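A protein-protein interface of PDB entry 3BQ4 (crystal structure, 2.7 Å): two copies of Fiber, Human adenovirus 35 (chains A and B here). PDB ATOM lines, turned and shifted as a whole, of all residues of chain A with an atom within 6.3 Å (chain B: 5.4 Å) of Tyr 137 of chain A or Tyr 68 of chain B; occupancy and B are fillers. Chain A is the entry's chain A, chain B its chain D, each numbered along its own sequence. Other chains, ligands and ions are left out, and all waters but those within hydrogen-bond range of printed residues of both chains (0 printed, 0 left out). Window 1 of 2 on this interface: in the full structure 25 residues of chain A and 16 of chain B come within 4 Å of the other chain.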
ATOM      1  N   LEU A  64      12.634  11.966  -5.481  1.00  0.00           N
ATOM      2  CA  LEU A  64      13.078  12.116  -4.099  1.00  0.00           C
ATOM      3  C   LEU A  64      12.749  10.919  -3.241  1.00  0.00           C
ATOM      4  O   LEU A  64      12.024  10.017  -3.661  1.00  0.00           O
ATOM      5  CB  LEU A  64      12.440  13.358  -3.468  1.00  0.00           C
ATOM      6  CG  LEU A  64      12.845  14.771  -3.996  1.00  0.00           C
ATOM      7  CD1 LEU A  64      11.971  15.837  -3.336  1.00  0.00           C
ATOM      8  CD2 LEU A  64      14.301  15.020  -3.730  1.00  0.00           C
ATOM      9  N   PRO A 132      20.730   7.015  -2.046  1.00  0.00           N
ATOM     10  CA  PRO A 132      20.994   8.411  -2.395  1.00  0.00           C
ATOM     11  C   PRO A 132      21.884   8.573  -3.634  1.00  0.00           C
ATOM     12  O   PRO A 132      23.048   8.147  -3.641  1.00  0.00           O
ATOM     13  CB  PRO A 132      21.655   8.965  -1.123  1.00  0.00           C
ATOM     14  CG  PRO A 132      22.405   7.790  -0.595  1.00  0.00           C
ATOM     15  CD  PRO A 132      21.416   6.644  -0.793  1.00  0.00           C
ATOM     16  N   SER A 133      21.328   9.197  -4.671  1.00  0.00           N
ATOM     17  CA  SER A 133      22.040   9.445  -5.929  1.00  0.00           C
ATOM     18  C   SER A 133      23.500   9.873  -5.726  1.00  0.00           C
ATOM     19  O   SER A 133      23.768  10.933  -5.165  1.00  0.00           O
ATOM     20  CB  SER A 133      21.305  10.528  -6.733  1.00  0.00           C
ATOM     21  OG  SER A 133      22.059  10.933  -7.864  1.00  0.00           O
ATOM     22  N   THR A 134      24.441   9.054  -6.192  1.00  0.00           N
ATOM     23  CA  THR A 134      25.866   9.368  -6.057  1.00  0.00           C
ATOM     24  C   THR A 134      26.306  10.376  -7.108  1.00  0.00           C
ATOM     25  O   THR A 134      27.488  10.454  -7.433  1.00  0.00           O
ATOM     26  CB  THR A 134      26.747   8.149  -6.257  1.00  0.00           C
ATOM     27  OG1 THR A 134      26.639   7.722  -7.618  1.00  0.00           O
ATOM     28  CG2 THR A 134      26.335   7.028  -5.332  1.00  0.00           C
ATOM     29  N   THR A 135      25.357  11.119  -7.665  1.00  0.00           N
ATOM     30  CA  THR A 135      25.689  12.133  -8.651  1.00  0.00           C
ATOM     31  C   THR A 135      25.457  13.521  -8.037  1.00  0.00           C
ATOM     32  O   THR A 135      26.185  14.468  -8.334  1.00  0.00           O
ATOM     33  CB  THR A 135      24.848  11.979  -9.940  1.00  0.00           C
ATOM     34  OG1 THR A 135      24.980  10.645 -10.442  1.00  0.00           O
ATOM     35  CG2 THR A 135      25.336  12.940 -11.006  1.00  0.00           C
ATOM     36  N   ALA A 136      24.455  13.647  -7.170  1.00  0.00           N
ATOM     37  CA  ALA A 136      24.180  14.931  -6.527  1.00  0.00           C
ATOM     38  C   ALA A 136      24.945  14.977  -5.220  1.00  0.00           C
ATOM     39  O   ALA A 136      25.116  16.036  -4.622  1.00  0.00           O
ATOM     40  CB  ALA A 136      22.693  15.081  -6.260  1.00  0.00           C
ATOM     41  N   TYR A 137      25.392  13.799  -4.792  1.00  0.00           N
ATOM     42  CA  TYR A 137      26.146  13.609  -3.553  1.00  0.00           C
ATOM     43  C   TYR A 137      27.333  12.672  -3.845  1.00  0.00           C
ATOM     44  O   TYR A 137      27.267  11.477  -3.546  1.00  0.00           O
ATOM     45  CB  TYR A 137      25.252  12.955  -2.495  1.00  0.00           C
ATOM     46  CG  TYR A 137      23.822  13.447  -2.471  1.00  0.00           C
ATOM     47  CD1 TYR A 137      22.752  12.565  -2.637  1.00  0.00           C
ATOM     48  CD2 TYR A 137      23.534  14.782  -2.262  1.00  0.00           C
ATOM     49  CE1 TYR A 137      21.433  13.007  -2.593  1.00  0.00           C
ATOM     50  CE2 TYR A 137      22.218  15.235  -2.214  1.00  0.00           C
ATOM     51  CZ  TYR A 137      21.172  14.346  -2.378  1.00  0.00           C
ATOM     52  OH  TYR A 137      19.872  14.804  -2.302  1.00  0.00           O
ATOM     53  N   PRO A 138      28.427  13.200  -4.437  1.00  0.00           N
ATOM     54  CA  PRO A 138      29.627  12.417  -4.776  1.00  0.00           C
ATOM     55  C   PRO A 138      30.410  11.883  -3.584  1.00  0.00           C
ATOM     56  O   PRO A 138      30.152  12.239  -2.437  1.00  0.00           O
ATOM     57  CB  PRO A 138      30.471  13.393  -5.590  1.00  0.00           C
ATOM     58  CG  PRO A 138      29.478  14.332  -6.140  1.00  0.00           C
ATOM     59  CD  PRO A 138      28.545  14.561  -4.983  1.00  0.00           C
ATOM     60  N   PHE A 139      31.384  11.030  -3.882  1.00  0.00           N
ATOM     61  CA  PHE A 139      32.224  10.425  -2.863  1.00  0.00           C
ATOM     62  C   PHE A 139      33.529  11.163  -2.634  1.00  0.00           C
ATOM     63  O   PHE A 139      33.874  12.098  -3.366  1.00  0.00           O
ATOM     64  CB  PHE A 139      32.561   8.976  -3.221  1.00  0.00           C
ATOM     65  CG  PHE A 139      31.597   7.979  -2.667  1.00  0.00           C
ATOM     66  CD1 PHE A 139      30.505   7.569  -3.407  1.00  0.00           C
ATOM     67  CD2 PHE A 139      31.768   7.473  -1.383  1.00  0.00           C
ATOM     68  CE1 PHE A 139      29.594   6.670  -2.882  1.00  0.00           C
ATOM     69  CE2 PHE A 139      30.862   6.575  -0.851  1.00  0.00           C
ATOM     70  CZ  PHE A 139      29.769   6.172  -1.607  1.00  0.00           C
ATOM     71  N   ARG A 144      34.516  19.681  -4.414  1.00  0.00           N
ATOM     72  CA  ARG A 144      33.084  19.590  -4.134  1.00  0.00           C
ATOM     73  C   ARG A 144      32.947  19.366  -2.631  1.00  0.00           C
ATOM     74  O   ARG A 144      31.954  18.818  -2.152  1.00  0.00           O
ATOM     75  CB  ARG A 144      32.465  18.418  -4.901  1.00  0.00           C
ATOM     76  CG  ARG A 144      32.215  18.715  -6.367  1.00  0.00           C
ATOM     77  CD  ARG A 144      31.120  19.759  -6.508  1.00  0.00           C
ATOM     78  NE  ARG A 144      29.857  19.273  -5.957  1.00  0.00           N
ATOM     79  CZ  ARG A 144      29.168  18.256  -6.466  1.00  0.00           C
ATOM     80  NH1 ARG A 144      29.620  17.617  -7.538  1.00  0.00           N
ATOM     81  NH2 ARG A 144      28.031  17.878  -5.903  1.00  0.00           N
ATOM     82  N   GLU A 147      29.120  19.994   0.964  1.00  0.00           N
ATOM     83  CA  GLU A 147      27.876  20.543   0.400  1.00  0.00           C
ATOM     84  C   GLU A 147      26.772  19.501   0.193  1.00  0.00           C
ATOM     85  O   GLU A 147      25.677  19.821  -0.275  1.00  0.00           O
ATOM     86  CB  GLU A 147      28.141  21.322  -0.905  1.00  0.00           C
ATOM     87  CG  GLU A 147      28.716  20.537  -2.076  1.00  0.00           C
ATOM     88  CD  GLU A 147      28.960  21.426  -3.288  1.00  0.00           C
ATOM     89  OE1 GLU A 147      29.686  22.433  -3.139  1.00  0.00           O
ATOM     90  OE2 GLU A 147      28.430  21.121  -4.379  1.00  0.00           O
ATOM     91  N   ASN A 148      27.068  18.250   0.540  1.00  0.00           N
ATOM     92  CA  ASN A 148      26.091  17.186   0.440  1.00  0.00           C
ATOM     93  C   ASN A 148      25.795  16.719   1.860  1.00  0.00           C
ATOM     94  O   ASN A 148      26.017  15.575   2.215  1.00  0.00           O
ATOM     95  CB  ASN A 148      26.592  16.027  -0.438  1.00  0.00           C
ATOM     96  CG  ASN A 148      27.786  15.321   0.140  1.00  0.00           C
ATOM     97  OD1 ASN A 148      28.174  14.250  -0.334  1.00  0.00           O
ATOM     98  ND2 ASN A 148      28.386  15.916   1.161  1.00  0.00           N
ATOM     99  N   TYR A 149      25.297  17.656   2.656  1.00  0.00           N
ATOM    100  CA  TYR A 149      24.921  17.432   4.043  1.00  0.00           C
ATOM    101  C   TYR A 149      23.511  18.000   4.270  1.00  0.00           C
ATOM    102  O   TYR A 149      23.136  19.016   3.678  1.00  0.00           O
ATOM    103  CB  TYR A 149      25.870  18.184   4.978  1.00  0.00           C
ATOM    104  CG  TYR A 149      27.174  17.509   5.324  1.00  0.00           C
ATOM    105  CD1 TYR A 149      28.301  17.648   4.511  1.00  0.00           C
ATOM    106  CD2 TYR A 149      27.297  16.778   6.501  1.00  0.00           C
ATOM    107  CE1 TYR A 149      29.528  17.078   4.871  1.00  0.00           C
ATOM    108  CE2 TYR A 149      28.509  16.204   6.870  1.00  0.00           C
ATOM    109  CZ  TYR A 149      29.624  16.357   6.058  1.00  0.00           C
ATOM    110  OH  TYR A 149      30.820  15.790   6.462  1.00  0.00           O
ATOM    111  N   ILE A 150      22.729  17.359   5.124  1.00  0.00           N
ATOM    112  CA  ILE A 150      21.405  17.883   5.413  1.00  0.00           C
ATOM    113  C   ILE A 150      21.381  18.271   6.890  1.00  0.00           C
ATOM    114  O   ILE A 150      21.396  17.417   7.769  1.00  0.00           O
ATOM    115  CB  ILE A 150      20.295  16.849   5.076  1.00  0.00           C
ATOM    116  CG1 ILE A 150      20.068  16.825   3.557  1.00  0.00           C
ATOM    117  CG2 ILE A 150      19.005  17.202   5.804  1.00  0.00           C
ATOM    118  CD1 ILE A 150      19.281  15.636   3.065  1.00  0.00           C
ATOM    119  N   MET A 172      24.822  13.071   6.581  1.00  0.00           N
ATOM    120  CA  MET A 172      25.896  13.087   5.607  1.00  0.00           C
ATOM    121  C   MET A 172      25.529  12.763   4.172  1.00  0.00           C
ATOM    122  O   MET A 172      25.349  13.676   3.371  1.00  0.00           O
ATOM    123  CB  MET A 172      27.001  12.163   6.077  1.00  0.00           C
ATOM    124  CG  MET A 172      28.177  12.905   6.683  1.00  0.00           C
ATOM    125  SD  MET A 172      29.576  13.129   5.534  1.00  0.00           S
ATOM    126  CE  MET A 172      28.770  13.897   4.169  1.00  0.00           C
ATOM    127  N   LEU A 173      25.425  11.474   3.843  1.00  0.00           N
ATOM    128  CA  LEU A 173      25.103  10.989   2.465  1.00  0.00           C
ATOM    129  C   LEU A 173      26.355  10.686   1.650  1.00  0.00           C
ATOM    130  O   LEU A 173      26.976  11.580   1.079  1.00  0.00           O
ATOM    131  CB  LEU A 173      24.251  11.977   1.628  1.00  0.00           C
ATOM    132  CG  LEU A 173      22.806  12.281   2.019  1.00  0.00           C
ATOM    133  CD1 LEU A 173      22.204  13.231   1.020  1.00  0.00           C
ATOM    134  CD2 LEU A 173      22.021  10.988   2.084  1.00  0.00           C
ATOM    135  N   ASN A 174      26.720   9.417   1.587  1.00  0.00           N
ATOM    136  CA  ASN A 174      27.880   9.023   0.829  1.00  0.00           C
ATOM    137  C   ASN A 174      29.100   9.797   1.291  1.00  0.00           C
ATOM    138  O   ASN A 174      29.655  10.599   0.545  1.00  0.00           O
ATOM    139  CB  ASN A 174      27.623   9.263  -0.661  1.00  0.00           C
ATOM    140  CG  ASN A 174      26.480   8.420  -1.195  1.00  0.00           C
ATOM    141  OD1 ASN A 174      26.157   7.371  -0.631  1.00  0.00           O
ATOM    142  ND2 ASN A 174      25.869   8.863  -2.291  1.00  0.00           N
ATOM    143  N   SER A 213      14.692  14.628   2.905  1.00  0.00           N
ATOM    144  CA  SER A 213      14.458  14.159   1.553  1.00  0.00           C
ATOM    145  C   SER A 213      15.712  14.402   0.724  1.00  0.00           C
ATOM    146  O   SER A 213      16.330  15.453   0.820  1.00  0.00           O
ATOM    147  CB  SER A 213      13.290  14.917   0.925  1.00  0.00           C
ATOM    148  OG  SER A 213      12.109  14.729   1.677  1.00  0.00           O
ATOM    149  N   TYR A 214      16.081  13.426  -0.092  1.00  0.00           N
ATOM    150  CA  TYR A 214      17.248  13.543  -0.958  1.00  0.00           C
ATOM    151  C   TYR A 214      16.905  12.945  -2.306  1.00  0.00           C
ATOM    152  O   TYR A 214      15.882  12.278  -2.450  1.00  0.00           O
ATOM    153  CB  TYR A 214      18.455  12.818  -0.345  1.00  0.00           C
ATOM    154  CG  TYR A 214      18.239  11.348   0.016  1.00  0.00           C
ATOM    155  CD1 TYR A 214      18.352  10.350  -0.942  1.00  0.00           C
ATOM    156  CD2 TYR A 214      18.007  10.960   1.329  1.00  0.00           C
ATOM    157  CE1 TYR A 214      18.260   9.008  -0.606  1.00  0.00           C
ATOM    158  CE2 TYR A 214      17.909   9.634   1.674  1.00  0.00           C
ATOM    159  CZ  TYR A 214      18.042   8.654   0.709  1.00  0.00           C
ATOM    160  OH  TYR A 214      17.987   7.311   1.057  1.00  0.00           O
ATOM    161  N   ILE A 215      17.771  13.180  -3.288  1.00  0.00           N
ATOM    162  CA  ILE A 215      17.579  12.678  -4.653  1.00  0.00           C
ATOM    163  C   ILE A 215      17.947  11.219  -4.823  1.00  0.00           C
ATOM    164  O   ILE A 215      19.115  10.894  -4.866  1.00  0.00           O
ATOM    165  CB  ILE A 215      18.441  13.432  -5.683  1.00  0.00           C
ATOM    166  CG1 ILE A 215      17.891  14.838  -5.937  1.00  0.00           C
ATOM    167  CG2 ILE A 215      18.504  12.606  -6.956  1.00  0.00           C
ATOM    168  CD1 ILE A 215      17.902  15.729  -4.731  1.00  0.00           C
ATOM    169  N   THR A 216      16.955  10.352  -4.952  1.00  0.00           N
ATOM    170  CA  THR A 216      17.207   8.929  -5.139  1.00  0.00           C
ATOM    171  C   THR A 216      18.128   8.615  -6.330  1.00  0.00           C
ATOM    172  O   THR A 216      18.307   9.441  -7.228  1.00  0.00           O
ATOM    173  CB  THR A 216      15.893   8.173  -5.366  1.00  0.00           C
ATOM    174  OG1 THR A 216      16.181   6.827  -5.758  1.00  0.00           O
ATOM    175  CG2 THR A 216      15.079   8.837  -6.470  1.00  0.00           C
ATOM    176  N   THR B  55      18.839  23.937  -7.604  1.00  0.00           N
ATOM    177  CA  THR B  55      18.492  22.525  -7.714  1.00  0.00           C
ATOM    178  C   THR B  55      17.103  22.444  -7.108  1.00  0.00           C
ATOM    179  O   THR B  55      16.956  22.521  -5.902  1.00  0.00           O
ATOM    180  CB  THR B  55      19.446  21.626  -6.923  1.00  0.00           C
ATOM    181  OG1 THR B  55      20.729  21.635  -7.557  1.00  0.00           O
ATOM    182  CG2 THR B  55      18.915  20.204  -6.884  1.00  0.00           C
ATOM    183  N   LEU B  56      16.084  22.313  -7.947  1.00  0.00           N
ATOM    184  CA  LEU B  56      14.724  22.252  -7.441  1.00  0.00           C
ATOM    185  C   LEU B  56      14.037  20.974  -7.887  1.00  0.00           C
ATOM    186  O   LEU B  56      13.992  20.675  -9.080  1.00  0.00           O
ATOM    187  CB  LEU B  56      13.950  23.477  -7.926  1.00  0.00           C
ATOM    188  CG  LEU B  56      12.480  23.662  -7.556  1.00  0.00           C
ATOM    189  CD1 LEU B  56      12.265  23.690  -6.062  1.00  0.00           C
ATOM    190  CD2 LEU B  56      12.029  24.961  -8.160  1.00  0.00           C
ATOM    191  N   VAL B  57      13.519  20.220  -6.919  1.00  0.00           N
ATOM    192  CA  VAL B  57      12.830  18.967  -7.201  1.00  0.00           C
ATOM    193  C   VAL B  57      11.401  18.954  -6.643  1.00  0.00           C
ATOM    194  O   VAL B  57      11.207  18.826  -5.438  1.00  0.00           O
ATOM    195  CB  VAL B  57      13.602  17.786  -6.604  1.00  0.00           C
ATOM    196  CG1 VAL B  57      12.812  16.508  -6.775  1.00  0.00           C
ATOM    197  CG2 VAL B  57      14.965  17.671  -7.265  1.00  0.00           C
ATOM    198  N   ASN B  66       5.803  17.976  -3.112  1.00  0.00           N
ATOM    199  CA  ASN B  66       6.988  17.841  -2.241  1.00  0.00           C
ATOM    200  C   ASN B  66       8.209  18.598  -2.708  1.00  0.00           C
ATOM    201  O   ASN B  66       8.814  18.286  -3.731  1.00  0.00           O
ATOM    202  CB  ASN B  66       7.364  16.386  -2.035  1.00  0.00           C
ATOM    203  CG  ASN B  66       6.697  15.814  -0.842  1.00  0.00           C
ATOM    204  OD1 ASN B  66       5.939  16.501  -0.163  1.00  0.00           O
ATOM    205  ND2 ASN B  66       6.969  14.557  -0.560  1.00  0.00           N
ATOM    206  N   GLY B  67       8.573  19.597  -1.928  1.00  0.00           N
ATOM    207  CA  GLY B  67       9.688  20.422  -2.304  1.00  0.00           C
ATOM    208  C   GLY B  67      11.019  20.024  -1.738  1.00  0.00           C
ATOM    209  O   GLY B  67      11.121  19.408  -0.678  1.00  0.00           O
ATOM    210  N   TYR B  68      12.036  20.392  -2.499  1.00  0.00           N
ATOM    211  CA  TYR B  68      13.418  20.168  -2.175  1.00  0.00           C
ATOM    212  C   TYR B  68      14.178  21.291  -2.907  1.00  0.00           C
ATOM    213  O   TYR B  68      14.221  21.323  -4.140  1.00  0.00           O
ATOM    214  CB  TYR B  68      13.863  18.805  -2.671  1.00  0.00           C
ATOM    215  CG  TYR B  68      15.329  18.589  -2.464  1.00  0.00           C
ATOM    216  CD1 TYR B  68      15.799  17.868  -1.377  1.00  0.00           C
ATOM    217  CD2 TYR B  68      16.257  19.138  -3.343  1.00  0.00           C
ATOM    218  CE1 TYR B  68      17.171  17.694  -1.178  1.00  0.00           C
ATOM    219  CE2 TYR B  68      17.608  18.978  -3.154  1.00  0.00           C
ATOM    220  CZ  TYR B  68      18.064  18.256  -2.082  1.00  0.00           C
ATOM    221  OH  TYR B  68      19.415  18.077  -1.947  1.00  0.00           O
ATOM    222  N   VAL B  69      14.774  22.204  -2.143  1.00  0.00           N
ATOM    223  CA  VAL B  69      15.498  23.344  -2.703  1.00  0.00           C
ATOM    224  C   VAL B  69      16.921  23.509  -2.169  1.00  0.00           C
ATOM    225  O   VAL B  69      17.162  23.354  -0.972  1.00  0.00           O
ATOM    226  CB  VAL B  69      14.702  24.632  -2.431  1.00  0.00           C
ATOM    227  CG1 VAL B  69      15.425  25.840  -2.966  1.00  0.00           C
ATOM    228  CG2 VAL B  69      13.346  24.508  -3.080  1.00  0.00           C
ATOM    229  N   SER B  70      17.858  23.834  -3.058  1.00  0.00           N
ATOM    230  CA  SER B  70      19.257  24.030  -2.675  1.00  0.00           C
ATOM    231  C   SER B  70      20.000  24.864  -3.705  1.00  0.00           C
ATOM    232  O   SER B  70      19.947  24.561  -4.894  1.00  0.00           O
ATOM    233  CB  SER B  70      19.958  22.681  -2.546  1.00  0.00           C
ATOM    234  OG  SER B  70      20.051  22.035  -3.804  1.00  0.00           O
ATOM    235  N   PRO B 209      19.874  21.859   1.736  1.00  0.00           N
ATOM    236  CA  PRO B 209      18.511  21.527   1.319  1.00  0.00           C
ATOM    237  C   PRO B 209      17.379  21.991   2.252  1.00  0.00           C
ATOM    238  O   PRO B 209      17.449  21.802   3.470  1.00  0.00           O
ATOM    239  CB  PRO B 209      18.545  19.994   1.202  1.00  0.00           C
ATOM    240  CG  PRO B 209      19.985  19.670   0.934  1.00  0.00           C
ATOM    241  CD  PRO B 209      20.699  20.640   1.864  1.00  0.00           C
ATOM    242  N   PHE B 210      16.338  22.595   1.675  1.00  0.00           N
ATOM    243  CA  PHE B 210      15.186  22.992   2.466  1.00  0.00           C
ATOM    244  C   PHE B 210      13.949  22.216   2.007  1.00  0.00           C
ATOM    245  O   PHE B 210      13.392  22.503   0.958  1.00  0.00           O
ATOM    246  CB  PHE B 210      14.908  24.491   2.352  1.00  0.00           C
ATOM    247  CG  PHE B 210      13.731  24.951   3.185  1.00  0.00           C
ATOM    248  CD1 PHE B 210      13.678  24.693   4.555  1.00  0.00           C
ATOM    249  CD2 PHE B 210      12.661  25.611   2.595  1.00  0.00           C
ATOM    250  CE1 PHE B 210      12.574  25.077   5.320  1.00  0.00           C
ATOM    251  CE2 PHE B 210      11.552  26.001   3.357  1.00  0.00           C
ATOM    252  CZ  PHE B 210      11.514  25.729   4.714  1.00  0.00           C
ATOM    253  N   PHE B 211      13.527  21.234   2.795  1.00  0.00           N
ATOM    254  CA  PHE B 211      12.349  20.434   2.486  1.00  0.00           C
ATOM    255  C   PHE B 211      11.087  21.257   2.765  1.00  0.00           C
ATOM    256  O   PHE B 211      11.031  21.959   3.782  1.00  0.00           O
ATOM    257  CB  PHE B 211      12.352  19.184   3.356  1.00  0.00           C
ATOM    258  CG  PHE B 211      13.715  18.539   3.470  1.00  0.00           C
ATOM    259  CD1 PHE B 211      14.257  18.248   4.737  1.00  0.00           C
ATOM    260  CD2 PHE B 211      14.485  18.272   2.336  1.00  0.00           C
ATOM    261  CE1 PHE B 211      15.541  17.709   4.862  1.00  0.00           C
ATOM    262  CE2 PHE B 211      15.765  17.735   2.462  1.00  0.00           C
ATOM    263  CZ  PHE B 211      16.289  17.456   3.728  1.00  0.00           C
ATOM    264  N   PHE B 212      10.092  21.159   1.866  1.00  0.00           N
ATOM    265  CA  PHE B 212       8.806  21.885   1.957  1.00  0.00           C
ATOM    266  C   PHE B 212       7.645  21.280   1.129  1.00  0.00           C
ATOM    267  O   PHE B 212       7.861  20.427   0.275  1.00  0.00           O
ATOM    268  CB  PHE B 212       9.000  23.327   1.506  1.00  0.00           C
ATOM    269  CG  PHE B 212       9.209  23.474   0.028  1.00  0.00           C
ATOM    270  CD1 PHE B 212       8.146  23.747  -0.823  1.00  0.00           C
ATOM    271  CD2 PHE B 212      10.470  23.312  -0.520  1.00  0.00           C
ATOM    272  CE1 PHE B 212       8.344  23.859  -2.207  1.00  0.00           C
ATOM    273  CE2 PHE B 212      10.669  23.423  -1.908  1.00  0.00           C
ATOM    274  CZ  PHE B 212       9.606  23.696  -2.744  1.00  0.00           C
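Tyr 137 of chain A touches just one residue of chain B: Tyr 68 (3.3 Å). Of the printed residues of chain A, Val 57 of chain B touches Leu 64 (3.3 Å). Tyr 68 of chain B touches just these residues of chain A: Leu 64, Tyr 137, Ser 213 and Ile 215. Of the printed residues of chain A, Phe 211 of chain B touches Ile 150 (3.4 Å) and Ser 213 (2.9 Å). The nearest printed residue of chain B that does not touch Tyr 137 of chain A is Pro 209 of chain B (5.8 Å). The nearest printed residue of chain B that does not touch Leu 64 of chain A is Asn 66 of chain B (4.02 Å).
N of Ser 133 of chain A sits at hydrogen-bond distance from O of Ile 215 of chain A, 2.8 Å away. The side-chain amide nitrogen (ND2) of Asn 174 of chain A sits at hydrogen-bond distance from the backbone carbonyl oxygen (O) of Tyr 137 of chain A, at 3.2 Å. The side-chain hydroxyl (OH) of Tyr 137 of chain A sits at hydrogen-bond distance from the backbone NH (N) of Ile 215 of chain A, at 2.8 Å. The side-chain sulfur (SD) of Met 172 of chain A lies within hydrogen-bond range of the side-chain hydroxyl (OH) of Tyr 149 of chain A (3.1 Å). The backbone carbonyl oxygen (O) of Tyr 68 of chain B is in hydrogen-bond range of the backbone NH (N) of Val 57 of chain B, 3.1 Å away.
OH of Tyr 137 of chain A sits at hydrogen-bond distance from OH of Tyr 68 of chain B (3.3 Å).
CG of Leu 64 of chain A touches CG1 of Val 57 of chain B, 3.3 Å away. CD1 of Leu 64 of chain A touches CB of Tyr 68 of chain B, at 3.6 Å. O of Tyr 149 of chain A touches CD of Pro 209 of chain B (3.4 Å). Ile 150 of chain A touches Pro 209 of chain B (CG1 to CG, 3.9 Å). Phe 211 of chain B touches Ile 150 of chain A (CZ to CG2, 3.4 Å). Ser 213 of chain A touches Tyr 68 of chain B. Ser 213 of chain A touches Phe 211 of chain B. Ile 215 of chain A touches Tyr 68 of chain B.
No position is printed for both chains. Of the 9 pairs that touch across the chains among the printed residues, none has its exchanged pair printed and touching as well.
Of the 12 printed residues of chain B, 4 touch a printed residue of chain A. Hydrophobic or aromatic side chains of chain B that line the printed part of chain A: Val 57, Tyr 68, Pro 209 and Phe 211. Hydrophobic or aromatic side chains of chain A that line the printed part of chain B: Leu 64, Tyr 137, Ile 150 and Ile 215. Along chain A the printed residues that touch a printed residue of chain B span positions 64 to 215. Among the printed residues, 9 pairs touch across the chains. Among the printed residues, no Asp or Glu carboxylate lies within 4 Å of a Lys or Arg side-chain nitrogen of the other chain.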
